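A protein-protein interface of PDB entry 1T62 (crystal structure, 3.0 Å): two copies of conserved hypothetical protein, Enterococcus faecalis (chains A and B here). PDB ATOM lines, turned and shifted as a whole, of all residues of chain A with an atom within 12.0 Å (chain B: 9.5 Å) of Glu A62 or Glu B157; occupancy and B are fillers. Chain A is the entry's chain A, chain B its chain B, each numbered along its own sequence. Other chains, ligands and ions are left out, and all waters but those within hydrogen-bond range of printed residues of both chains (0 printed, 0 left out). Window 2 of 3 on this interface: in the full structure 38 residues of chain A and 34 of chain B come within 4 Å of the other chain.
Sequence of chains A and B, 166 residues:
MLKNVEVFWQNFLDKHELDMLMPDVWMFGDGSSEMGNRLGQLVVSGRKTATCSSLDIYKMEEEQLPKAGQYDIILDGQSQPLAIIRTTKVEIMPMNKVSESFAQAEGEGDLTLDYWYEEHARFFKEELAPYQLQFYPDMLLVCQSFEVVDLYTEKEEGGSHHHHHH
The backbone carbonyl oxygen of Glu B157 lies close to the side-chain carboxylate of Glu A62, at 2.6 Å. OE1 of Glu A62 sits close to N of Gly B158.
N of Lys A59 lies within hydrogen-bond range of OE1 of Glu A63 (3.0 Å). A ring nitrogen (ND1) of His B161 lies within hydrogen-bond range of the backbone NH of Gly B159 (3.1 Å).
Among the printed residues, merely in contact across the chains: Lys A59 with Gly B158 (3.99 Å), Lys A59 with Gly B159 (3.3 Å), Glu A63 with Gly B159 (3.4 Å) and Glu A63 with Ser B160 (3.0 Å).
Tyr A58 touches none of the printed residues of chain B. Of the printed residues of chain B, Lys A59 touches Gly B158 and Gly B159. Glu A62 touches just these residues of chain B: Glu B157 and Gly B158. Printed residues of chain B within 4 Å of Glu A63: Gly B159 and Ser B160. Tyr B152 touches none of the printed residues of chain A. No residue of chain A comes within 4 Å of Glu B156. Printed residues of chain A within 4 Å of Gly B158: Lys A59 (3.99 Å) and Glu A62 (2.9 Å). Gly B159 touches just these residues of chain A: Lys A59 and Glu A63. Of the printed residues of chain A, Ser B160 touches Glu A63. The nearest residue of chain B that does not touch Glu A62 is Glu B156 (4.04 Å). The nearest printed residue of chain A that does not touch Ser B160 is Asp A24 (4.3 Å).
Of the 15 printed residues of chain A, 3 touch a printed residue of chain B. Along chain A the printed residues that touch a printed residue of chain B span positions 59 to 63. Among the printed residues, 6 pairs touch across the chains. Among the printed residues, no Asp or Glu carboxylate lies within 4 Å of a Lys or Arg side-chain nitrogen of the other chain.
No position is printed for both chains. Of the 6 pairs that touch across the chains among the printed residues, none has its exchanged pair printed and touching as well.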
ATOM      1  N   ASP A  24      18.613  14.834  20.426  1.00  0.00           N
ATOM      2  CA  ASP A  24      17.820  14.261  19.352  1.00  0.00           C
ATOM      3  C   ASP A  24      17.013  15.384  18.717  1.00  0.00           C
ATOM      4  O   ASP A  24      16.762  16.404  19.358  1.00  0.00           O
ATOM      5  CB  ASP A  24      16.891  13.182  19.913  1.00  0.00           C
ATOM      6  CG  ASP A  24      17.651  11.980  20.439  1.00  0.00           C
ATOM      7  OD1 ASP A  24      17.082  11.206  21.236  1.00  0.00           O
ATOM      8  OD2 ASP A  24      18.823  11.804  20.047  1.00  0.00           O
ATOM      9  N   LEU A  55       6.252   2.936  25.236  1.00  0.00           N
ATOM     10  CA  LEU A  55       7.353   2.311  25.965  1.00  0.00           C
ATOM     11  C   LEU A  55       7.792   1.011  25.302  1.00  0.00           C
ATOM     12  O   LEU A  55       8.972   0.827  25.022  1.00  0.00           O
ATOM     13  CB  LEU A  55       6.938   2.044  27.419  1.00  0.00           C
ATOM     14  CG  LEU A  55       7.859   1.251  28.355  1.00  0.00           C
ATOM     15  CD1 LEU A  55       7.699  -0.237  28.101  1.00  0.00           C
ATOM     16  CD2 LEU A  55       9.300   1.686  28.155  1.00  0.00           C
ATOM     17  N   ASP A  56       6.838   0.118  25.053  1.00  0.00           N
ATOM     18  CA  ASP A  56       7.116  -1.176  24.435  1.00  0.00           C
ATOM     19  C   ASP A  56       7.993  -1.093  23.190  1.00  0.00           C
ATOM     20  O   ASP A  56       8.815  -1.976  22.942  1.00  0.00           O
ATOM     21  CB  ASP A  56       5.804  -1.871  24.084  1.00  0.00           C
ATOM     22  CG  ASP A  56       5.000  -2.234  25.311  1.00  0.00           C
ATOM     23  OD1 ASP A  56       3.823  -2.623  25.160  1.00  0.00           O
ATOM     24  OD2 ASP A  56       5.548  -2.136  26.429  1.00  0.00           O
ATOM     25  N   ILE A  57       7.815  -0.028  22.415  1.00  0.00           N
ATOM     26  CA  ILE A  57       8.570   0.187  21.185  1.00  0.00           C
ATOM     27  C   ILE A  57      10.078   0.358  21.444  1.00  0.00           C
ATOM     28  O   ILE A  57      10.891   0.148  20.550  1.00  0.00           O
ATOM     29  CB  ILE A  57       8.000   1.426  20.421  1.00  0.00           C
ATOM     30  CG1 ILE A  57       7.990   1.179  18.912  1.00  0.00           C
ATOM     31  CG2 ILE A  57       8.824   2.658  20.726  1.00  0.00           C
ATOM     32  CD1 ILE A  57       9.363   1.111  18.282  1.00  0.00           C
ATOM     33  N   TYR A  58      10.451   0.741  22.665  1.00  0.00           N
ATOM     34  CA  TYR A  58      11.861   0.916  23.026  1.00  0.00           C
ATOM     35  C   TYR A  58      12.539  -0.448  23.137  1.00  0.00           C
ATOM     36  O   TYR A  58      11.933  -1.411  23.603  1.00  0.00           O
ATOM     37  CB  TYR A  58      11.983   1.662  24.368  1.00  0.00           C
ATOM     38  CG  TYR A  58      11.760   3.170  24.286  1.00  0.00           C
ATOM     39  CD1 TYR A  58      12.835   4.052  24.168  1.00  0.00           C
ATOM     40  CD2 TYR A  58      10.469   3.707  24.278  1.00  0.00           C
ATOM     41  CE1 TYR A  58      12.635   5.429  24.042  1.00  0.00           C
ATOM     42  CE2 TYR A  58      10.255   5.085  24.152  1.00  0.00           C
ATOM     43  CZ  TYR A  58      11.343   5.944  24.033  1.00  0.00           C
ATOM     44  OH  TYR A  58      11.134   7.312  23.911  1.00  0.00           O
ATOM     45  N   LYS A  59      13.793  -0.538  22.706  1.00  0.00           N
ATOM     46  CA  LYS A  59      14.528  -1.797  22.780  1.00  0.00           C
ATOM     47  C   LYS A  59      15.333  -1.863  24.083  1.00  0.00           C
ATOM     48  O   LYS A  59      16.493  -1.447  24.144  1.00  0.00           O
ATOM     49  CB  LYS A  59      15.423  -1.927  21.549  1.00  0.00           C
ATOM     50  CG  LYS A  59      14.626  -1.784  20.260  1.00  0.00           C
ATOM     51  CD  LYS A  59      15.487  -1.866  19.014  1.00  0.00           C
ATOM     52  CE  LYS A  59      15.756  -3.307  18.589  1.00  0.00           C
ATOM     53  NZ  LYS A  59      14.556  -3.971  17.983  1.00  0.00           N
ATOM     54  N   MET A  60      14.683  -2.385  25.124  1.00  0.00           N
ATOM     55  CA  MET A  60      15.246  -2.514  26.469  1.00  0.00           C
ATOM     56  C   MET A  60      16.715  -2.891  26.639  1.00  0.00           C
ATOM     57  O   MET A  60      17.325  -2.541  27.649  1.00  0.00           O
ATOM     58  CB  MET A  60      14.405  -3.493  27.285  1.00  0.00           C
ATOM     59  CG  MET A  60      13.055  -2.950  27.681  1.00  0.00           C
ATOM     60  SD  MET A  60      13.196  -1.557  28.823  1.00  0.00           S
ATOM     61  CE  MET A  60      12.891  -0.177  27.752  1.00  0.00           C
ATOM     62  N   GLU A  61      17.291  -3.612  25.687  1.00  0.00           N
ATOM     63  CA  GLU A  61      18.685  -3.990  25.829  1.00  0.00           C
ATOM     64  C   GLU A  61      19.649  -3.196  24.959  1.00  0.00           C
ATOM     65  O   GLU A  61      20.858  -3.221  25.191  1.00  0.00           O
ATOM     66  CB  GLU A  61      18.850  -5.481  25.556  1.00  0.00           C
ATOM     67  CG  GLU A  61      18.431  -6.372  26.718  1.00  0.00           C
ATOM     68  CD  GLU A  61      19.287  -6.171  27.974  1.00  0.00           C
ATOM     69  OE1 GLU A  61      20.534  -6.282  27.881  1.00  0.00           O
ATOM     70  OE2 GLU A  61      18.710  -5.908  29.058  1.00  0.00           O
ATOM     71  N   GLU A  62      19.116  -2.479  23.974  1.00  0.00           N
ATOM     72  CA  GLU A  62      19.934  -1.694  23.055  1.00  0.00           C
ATOM     73  C   GLU A  62      20.012  -0.205  23.362  1.00  0.00           C
ATOM     74  O   GLU A  62      20.932   0.470  22.903  1.00  0.00           O
ATOM     75  CB  GLU A  62      19.422  -1.870  21.626  1.00  0.00           C
ATOM     76  CG  GLU A  62      19.888  -3.126  20.917  1.00  0.00           C
ATOM     77  CD  GLU A  62      19.418  -3.168  19.465  1.00  0.00           C
ATOM     78  OE1 GLU A  62      19.529  -2.132  18.769  1.00  0.00           O
ATOM     79  OE2 GLU A  62      18.942  -4.237  19.015  1.00  0.00           O
ATOM     80  N   GLU A  63      19.049   0.308  24.124  1.00  0.00           N
ATOM     81  CA  GLU A  63      19.001   1.737  24.470  1.00  0.00           C
ATOM     82  C   GLU A  63      18.374   1.948  25.833  1.00  0.00           C
ATOM     83  O   GLU A  63      17.811   1.019  26.395  1.00  0.00           O
ATOM     84  CB  GLU A  63      18.159   2.495  23.449  1.00  0.00           C
ATOM     85  CG  GLU A  63      16.856   1.780  23.130  1.00  0.00           C
ATOM     86  CD  GLU A  63      15.854   2.642  22.397  1.00  0.00           C
ATOM     87  OE1 GLU A  63      14.898   2.067  21.831  1.00  0.00           O
ATOM     88  OE2 GLU A  63      16.012   3.882  22.401  1.00  0.00           O
ATOM     89  N   GLN A  64      18.462   3.166  26.360  1.00  0.00           N
ATOM     90  CA  GLN A  64      17.858   3.471  27.661  1.00  0.00           C
ATOM     91  C   GLN A  64      16.717   4.453  27.437  1.00  0.00           C
ATOM     92  O   GLN A  64      16.605   5.036  26.360  1.00  0.00           O
ATOM     93  CB  GLN A  64      18.890   4.069  28.627  1.00  0.00           C
ATOM     94  CG  GLN A  64      20.135   3.204  28.816  1.00  0.00           C
ATOM     95  CD  GLN A  64      21.072   3.721  29.895  1.00  0.00           C
ATOM     96  OE1 GLN A  64      21.281   4.924  30.037  1.00  0.00           O
ATOM     97  NE2 GLN A  64      21.656   2.804  30.645  1.00  0.00           N
ATOM     98  N   LEU A  65      15.867   4.635  28.440  1.00  0.00           N
ATOM     99  CA  LEU A  65      14.734   5.541  28.285  1.00  0.00           C
ATOM    100  C   LEU A  65      15.105   6.978  28.624  1.00  0.00           C
ATOM    101  O   LEU A  65      16.041   7.232  29.390  1.00  0.00           O
ATOM    102  CB  LEU A  65      13.557   5.116  29.175  1.00  0.00           C
ATOM    103  CG  LEU A  65      13.233   3.629  29.336  1.00  0.00           C
ATOM    104  CD1 LEU A  65      11.878   3.466  30.034  1.00  0.00           C
ATOM    105  CD2 LEU A  65      13.202   2.969  27.987  1.00  0.00           C
ATOM    106  N   PRO A  66      14.375   7.942  28.048  1.00  0.00           N
ATOM    107  CA  PRO A  66      14.641   9.357  28.314  1.00  0.00           C
ATOM    108  C   PRO A  66      14.689   9.638  29.817  1.00  0.00           C
ATOM    109  O   PRO A  66      13.828   9.186  30.578  1.00  0.00           O
ATOM    110  CB  PRO A  66      13.488  10.073  27.608  1.00  0.00           C
ATOM    111  CG  PRO A  66      12.449   8.987  27.375  1.00  0.00           C
ATOM    112  CD  PRO A  66      13.270   7.774  27.092  1.00  0.00           C
ATOM    113  N   LYS A  67      15.709  10.383  30.235  1.00  0.00           N
ATOM    114  CA  LYS A  67      15.917  10.716  31.635  1.00  0.00           C
ATOM    115  C   LYS A  67      15.722  12.205  31.882  1.00  0.00           C
ATOM    116  O   LYS A  67      15.840  13.025  30.964  1.00  0.00           O
ATOM    117  CB  LYS A  67      17.346  10.359  32.067  1.00  0.00           C
ATOM    118  CG  LYS A  67      17.878   8.985  31.680  1.00  0.00           C
ATOM    119  CD  LYS A  67      17.148   7.843  32.378  1.00  0.00           C
ATOM    120  CE  LYS A  67      18.107   6.703  32.732  1.00  0.00           C
ATOM    121  NZ  LYS A  67      19.020   6.375  31.599  1.00  0.00           N
ATOM    122  N   TYR A 131       4.904  -2.479  13.313  1.00  0.00           N
ATOM    123  CA  TYR A 131       5.719  -3.457  14.028  1.00  0.00           C
ATOM    124  C   TYR A 131       4.769  -4.580  14.454  1.00  0.00           C
ATOM    125  O   TYR A 131       3.794  -4.880  13.756  1.00  0.00           O
ATOM    126  CB  TYR A 131       6.358  -2.842  15.284  1.00  0.00           C
ATOM    127  CG  TYR A 131       6.926  -1.435  15.148  1.00  0.00           C
ATOM    128  CD1 TYR A 131       6.155  -0.314  15.472  1.00  0.00           C
ATOM    129  CD2 TYR A 131       8.249  -1.225  14.752  1.00  0.00           C
ATOM    130  CE1 TYR A 131       6.694   0.979  15.412  1.00  0.00           C
ATOM    131  CE2 TYR A 131       8.795   0.062  14.686  1.00  0.00           C
ATOM    132  CZ  TYR A 131       8.015   1.158  15.020  1.00  0.00           C
ATOM    133  OH  TYR A 131       8.562   2.425  14.983  1.00  0.00           O
ATOM    134  N   ASN B  11      31.799   5.828   8.231  1.00  0.00           N
ATOM    135  CA  ASN B  11      31.755   4.419   7.896  1.00  0.00           C
ATOM    136  C   ASN B  11      31.878   4.242   6.382  1.00  0.00           C
ATOM    137  O   ASN B  11      32.528   3.311   5.913  1.00  0.00           O
ATOM    138  CB  ASN B  11      30.448   3.770   8.375  1.00  0.00           C
ATOM    139  CG  ASN B  11      30.309   3.731   9.912  1.00  0.00           C
ATOM    140  OD1 ASN B  11      31.303   3.686  10.654  1.00  0.00           O
ATOM    141  ND2 ASN B  11      29.058   3.715  10.387  1.00  0.00           N
ATOM    142  N   TYR B 152      21.936   3.402   4.984  1.00  0.00           N
ATOM    143  CA  TYR B 152      22.227   3.611   6.402  1.00  0.00           C
ATOM    144  C   TYR B 152      21.670   2.455   7.189  1.00  0.00           C
ATOM    145  O   TYR B 152      20.521   2.491   7.610  1.00  0.00           O
ATOM    146  CB  TYR B 152      21.600   4.913   6.895  1.00  0.00           C
ATOM    147  CG  TYR B 152      21.817   5.214   8.367  1.00  0.00           C
ATOM    148  CD1 TYR B 152      20.842   4.901   9.315  1.00  0.00           C
ATOM    149  CD2 TYR B 152      22.984   5.854   8.810  1.00  0.00           C
ATOM    150  CE1 TYR B 152      21.017   5.226  10.674  1.00  0.00           C
ATOM    151  CE2 TYR B 152      23.172   6.182  10.167  1.00  0.00           C
ATOM    152  CZ  TYR B 152      22.182   5.868  11.091  1.00  0.00           C
ATOM    153  OH  TYR B 152      22.334   6.216  12.419  1.00  0.00           O
ATOM    154  N   THR B 153      22.495   1.431   7.375  1.00  0.00           N
ATOM    155  CA  THR B 153      22.110   0.237   8.108  1.00  0.00           C
ATOM    156  C   THR B 153      22.527   0.305   9.575  1.00  0.00           C
ATOM    157  O   THR B 153      22.308  -0.646  10.326  1.00  0.00           O
ATOM    158  CB  THR B 153      22.744  -1.020   7.492  1.00  0.00           C
ATOM    159  OG1 THR B 153      24.166  -0.854   7.436  1.00  0.00           O
ATOM    160  CG2 THR B 153      22.199  -1.273   6.097  1.00  0.00           C
ATOM    161  N   GLU B 154      23.148   1.412   9.982  1.00  0.00           N
ATOM    162  CA  GLU B 154      23.550   1.596  11.376  1.00  0.00           C
ATOM    163  C   GLU B 154      22.263   1.700  12.198  1.00  0.00           C
ATOM    164  O   GLU B 154      22.264   1.547  13.421  1.00  0.00           O
ATOM    165  CB  GLU B 154      24.364   2.884  11.532  1.00  0.00           C
ATOM    166  CG  GLU B 154      25.775   2.794  10.984  1.00  0.00           C
ATOM    167  CD  GLU B 154      25.867   2.986   9.480  1.00  0.00           C
ATOM    168  OE1 GLU B 154      24.909   2.636   8.755  1.00  0.00           O
ATOM    169  OE2 GLU B 154      26.921   3.478   9.021  1.00  0.00           O
ATOM    170  N   LYS B 155      21.170   1.957  11.478  1.00  0.00           N
ATOM    171  CA  LYS B 155      19.820   2.111  12.014  1.00  0.00           C
ATOM    172  C   LYS B 155      19.306   0.864  12.736  1.00  0.00           C
ATOM    173  O   LYS B 155      18.453   0.969  13.619  1.00  0.00           O
ATOM    174  CB  LYS B 155      18.864   2.464  10.865  1.00  0.00           C
ATOM    175  CG  LYS B 155      17.472   2.939  11.289  1.00  0.00           C
ATOM    176  CD  LYS B 155      16.587   3.249  10.069  1.00  0.00           C
ATOM    177  CE  LYS B 155      17.227   4.297   9.148  1.00  0.00           C
ATOM    178  NZ  LYS B 155      16.427   4.587   7.926  1.00  0.00           N
ATOM    179  N   GLU B 156      19.822  -0.306  12.362  1.00  0.00           N
ATOM    180  CA  GLU B 156      19.396  -1.566  12.975  1.00  0.00           C
ATOM    181  C   GLU B 156      20.123  -1.913  14.273  1.00  0.00           C
ATOM    182  O   GLU B 156      19.905  -2.990  14.841  1.00  0.00           O
ATOM    183  CB  GLU B 156      19.565  -2.729  11.991  1.00  0.00           C
ATOM    184  CG  GLU B 156      18.555  -2.754  10.856  1.00  0.00           C
ATOM    185  CD  GLU B 156      19.206  -2.577   9.490  1.00  0.00           C
ATOM    186  OE1 GLU B 156      20.085  -3.401   9.126  1.00  0.00           O
ATOM    187  OE2 GLU B 156      18.838  -1.612   8.777  1.00  0.00           O
ATOM    188  N   GLU B 157      20.960  -0.995  14.757  1.00  0.00           N
ATOM    189  CA  GLU B 157      21.730  -1.244  15.972  1.00  0.00           C
ATOM    190  C   GLU B 157      21.321  -0.434  17.216  1.00  0.00           C
ATOM    191  O   GLU B 157      21.695  -0.783  18.339  1.00  0.00           O
ATOM    192  CB  GLU B 157      23.208  -1.009  15.670  1.00  0.00           C
ATOM    193  CG  GLU B 157      23.673  -1.587  14.338  1.00  0.00           C
ATOM    194  CD  GLU B 157      23.940  -3.085  14.382  1.00  0.00           C
ATOM    195  OE1 GLU B 157      23.123  -3.831  14.970  1.00  0.00           O
ATOM    196  OE2 GLU B 157      24.972  -3.510  13.809  1.00  0.00           O
ATOM    197  N   GLY B 158      20.557   0.638  17.022  1.00  0.00           N
ATOM    198  CA  GLY B 158      20.133   1.455  18.150  1.00  0.00           C
ATOM    199  C   GLY B 158      18.748   1.128  18.687  1.00  0.00           C
ATOM    200  O   GLY B 158      18.623   0.495  19.731  1.00  0.00           O
ATOM    201  N   GLY B 159      17.709   1.563  17.973  1.00  0.00           N
ATOM    202  CA  GLY B 159      16.343   1.307  18.399  1.00  0.00           C
ATOM    203  C   GLY B 159      15.565   2.603  18.551  1.00  0.00           C
ATOM    204  O   GLY B 159      14.344   2.652  18.352  1.00  0.00           O
ATOM    205  N   SER B 160      16.296   3.655  18.919  1.00  0.00           N
ATOM    206  CA  SER B 160      15.733   4.992  19.107  1.00  0.00           C
ATOM    207  C   SER B 160      15.719   5.699  17.756  1.00  0.00           C
ATOM    208  O   SER B 160      16.081   6.872  17.644  1.00  0.00           O
ATOM    209  CB  SER B 160      16.584   5.796  20.108  1.00  0.00           C
ATOM    210  OG  SER B 160      16.063   7.103  20.335  1.00  0.00           O
ATOM    211  N   HIS B 161      15.310   4.966  16.729  1.00  0.00           N
ATOM    212  CA  HIS B 161      15.249   5.518  15.388  1.00  0.00           C
ATOM    213  C   HIS B 161      13.800   5.564  14.938  1.00  0.00           C
ATOM    214  O   HIS B 161      13.281   4.655  14.281  1.00  0.00           O
ATOM    215  CB  HIS B 161      16.129   4.690  14.452  1.00  0.00           C
ATOM    216  CG  HIS B 161      17.558   4.627  14.897  1.00  0.00           C
ATOM    217  ND1 HIS B 161      17.942   4.018  16.073  1.00  0.00           N
ATOM    218  CD2 HIS B 161      18.684   5.160  14.364  1.00  0.00           C
ATOM    219  CE1 HIS B 161      19.241   4.181  16.247  1.00  0.00           C
ATOM    220  NE2 HIS B 161      19.715   4.870  15.224  1.00  0.00           N
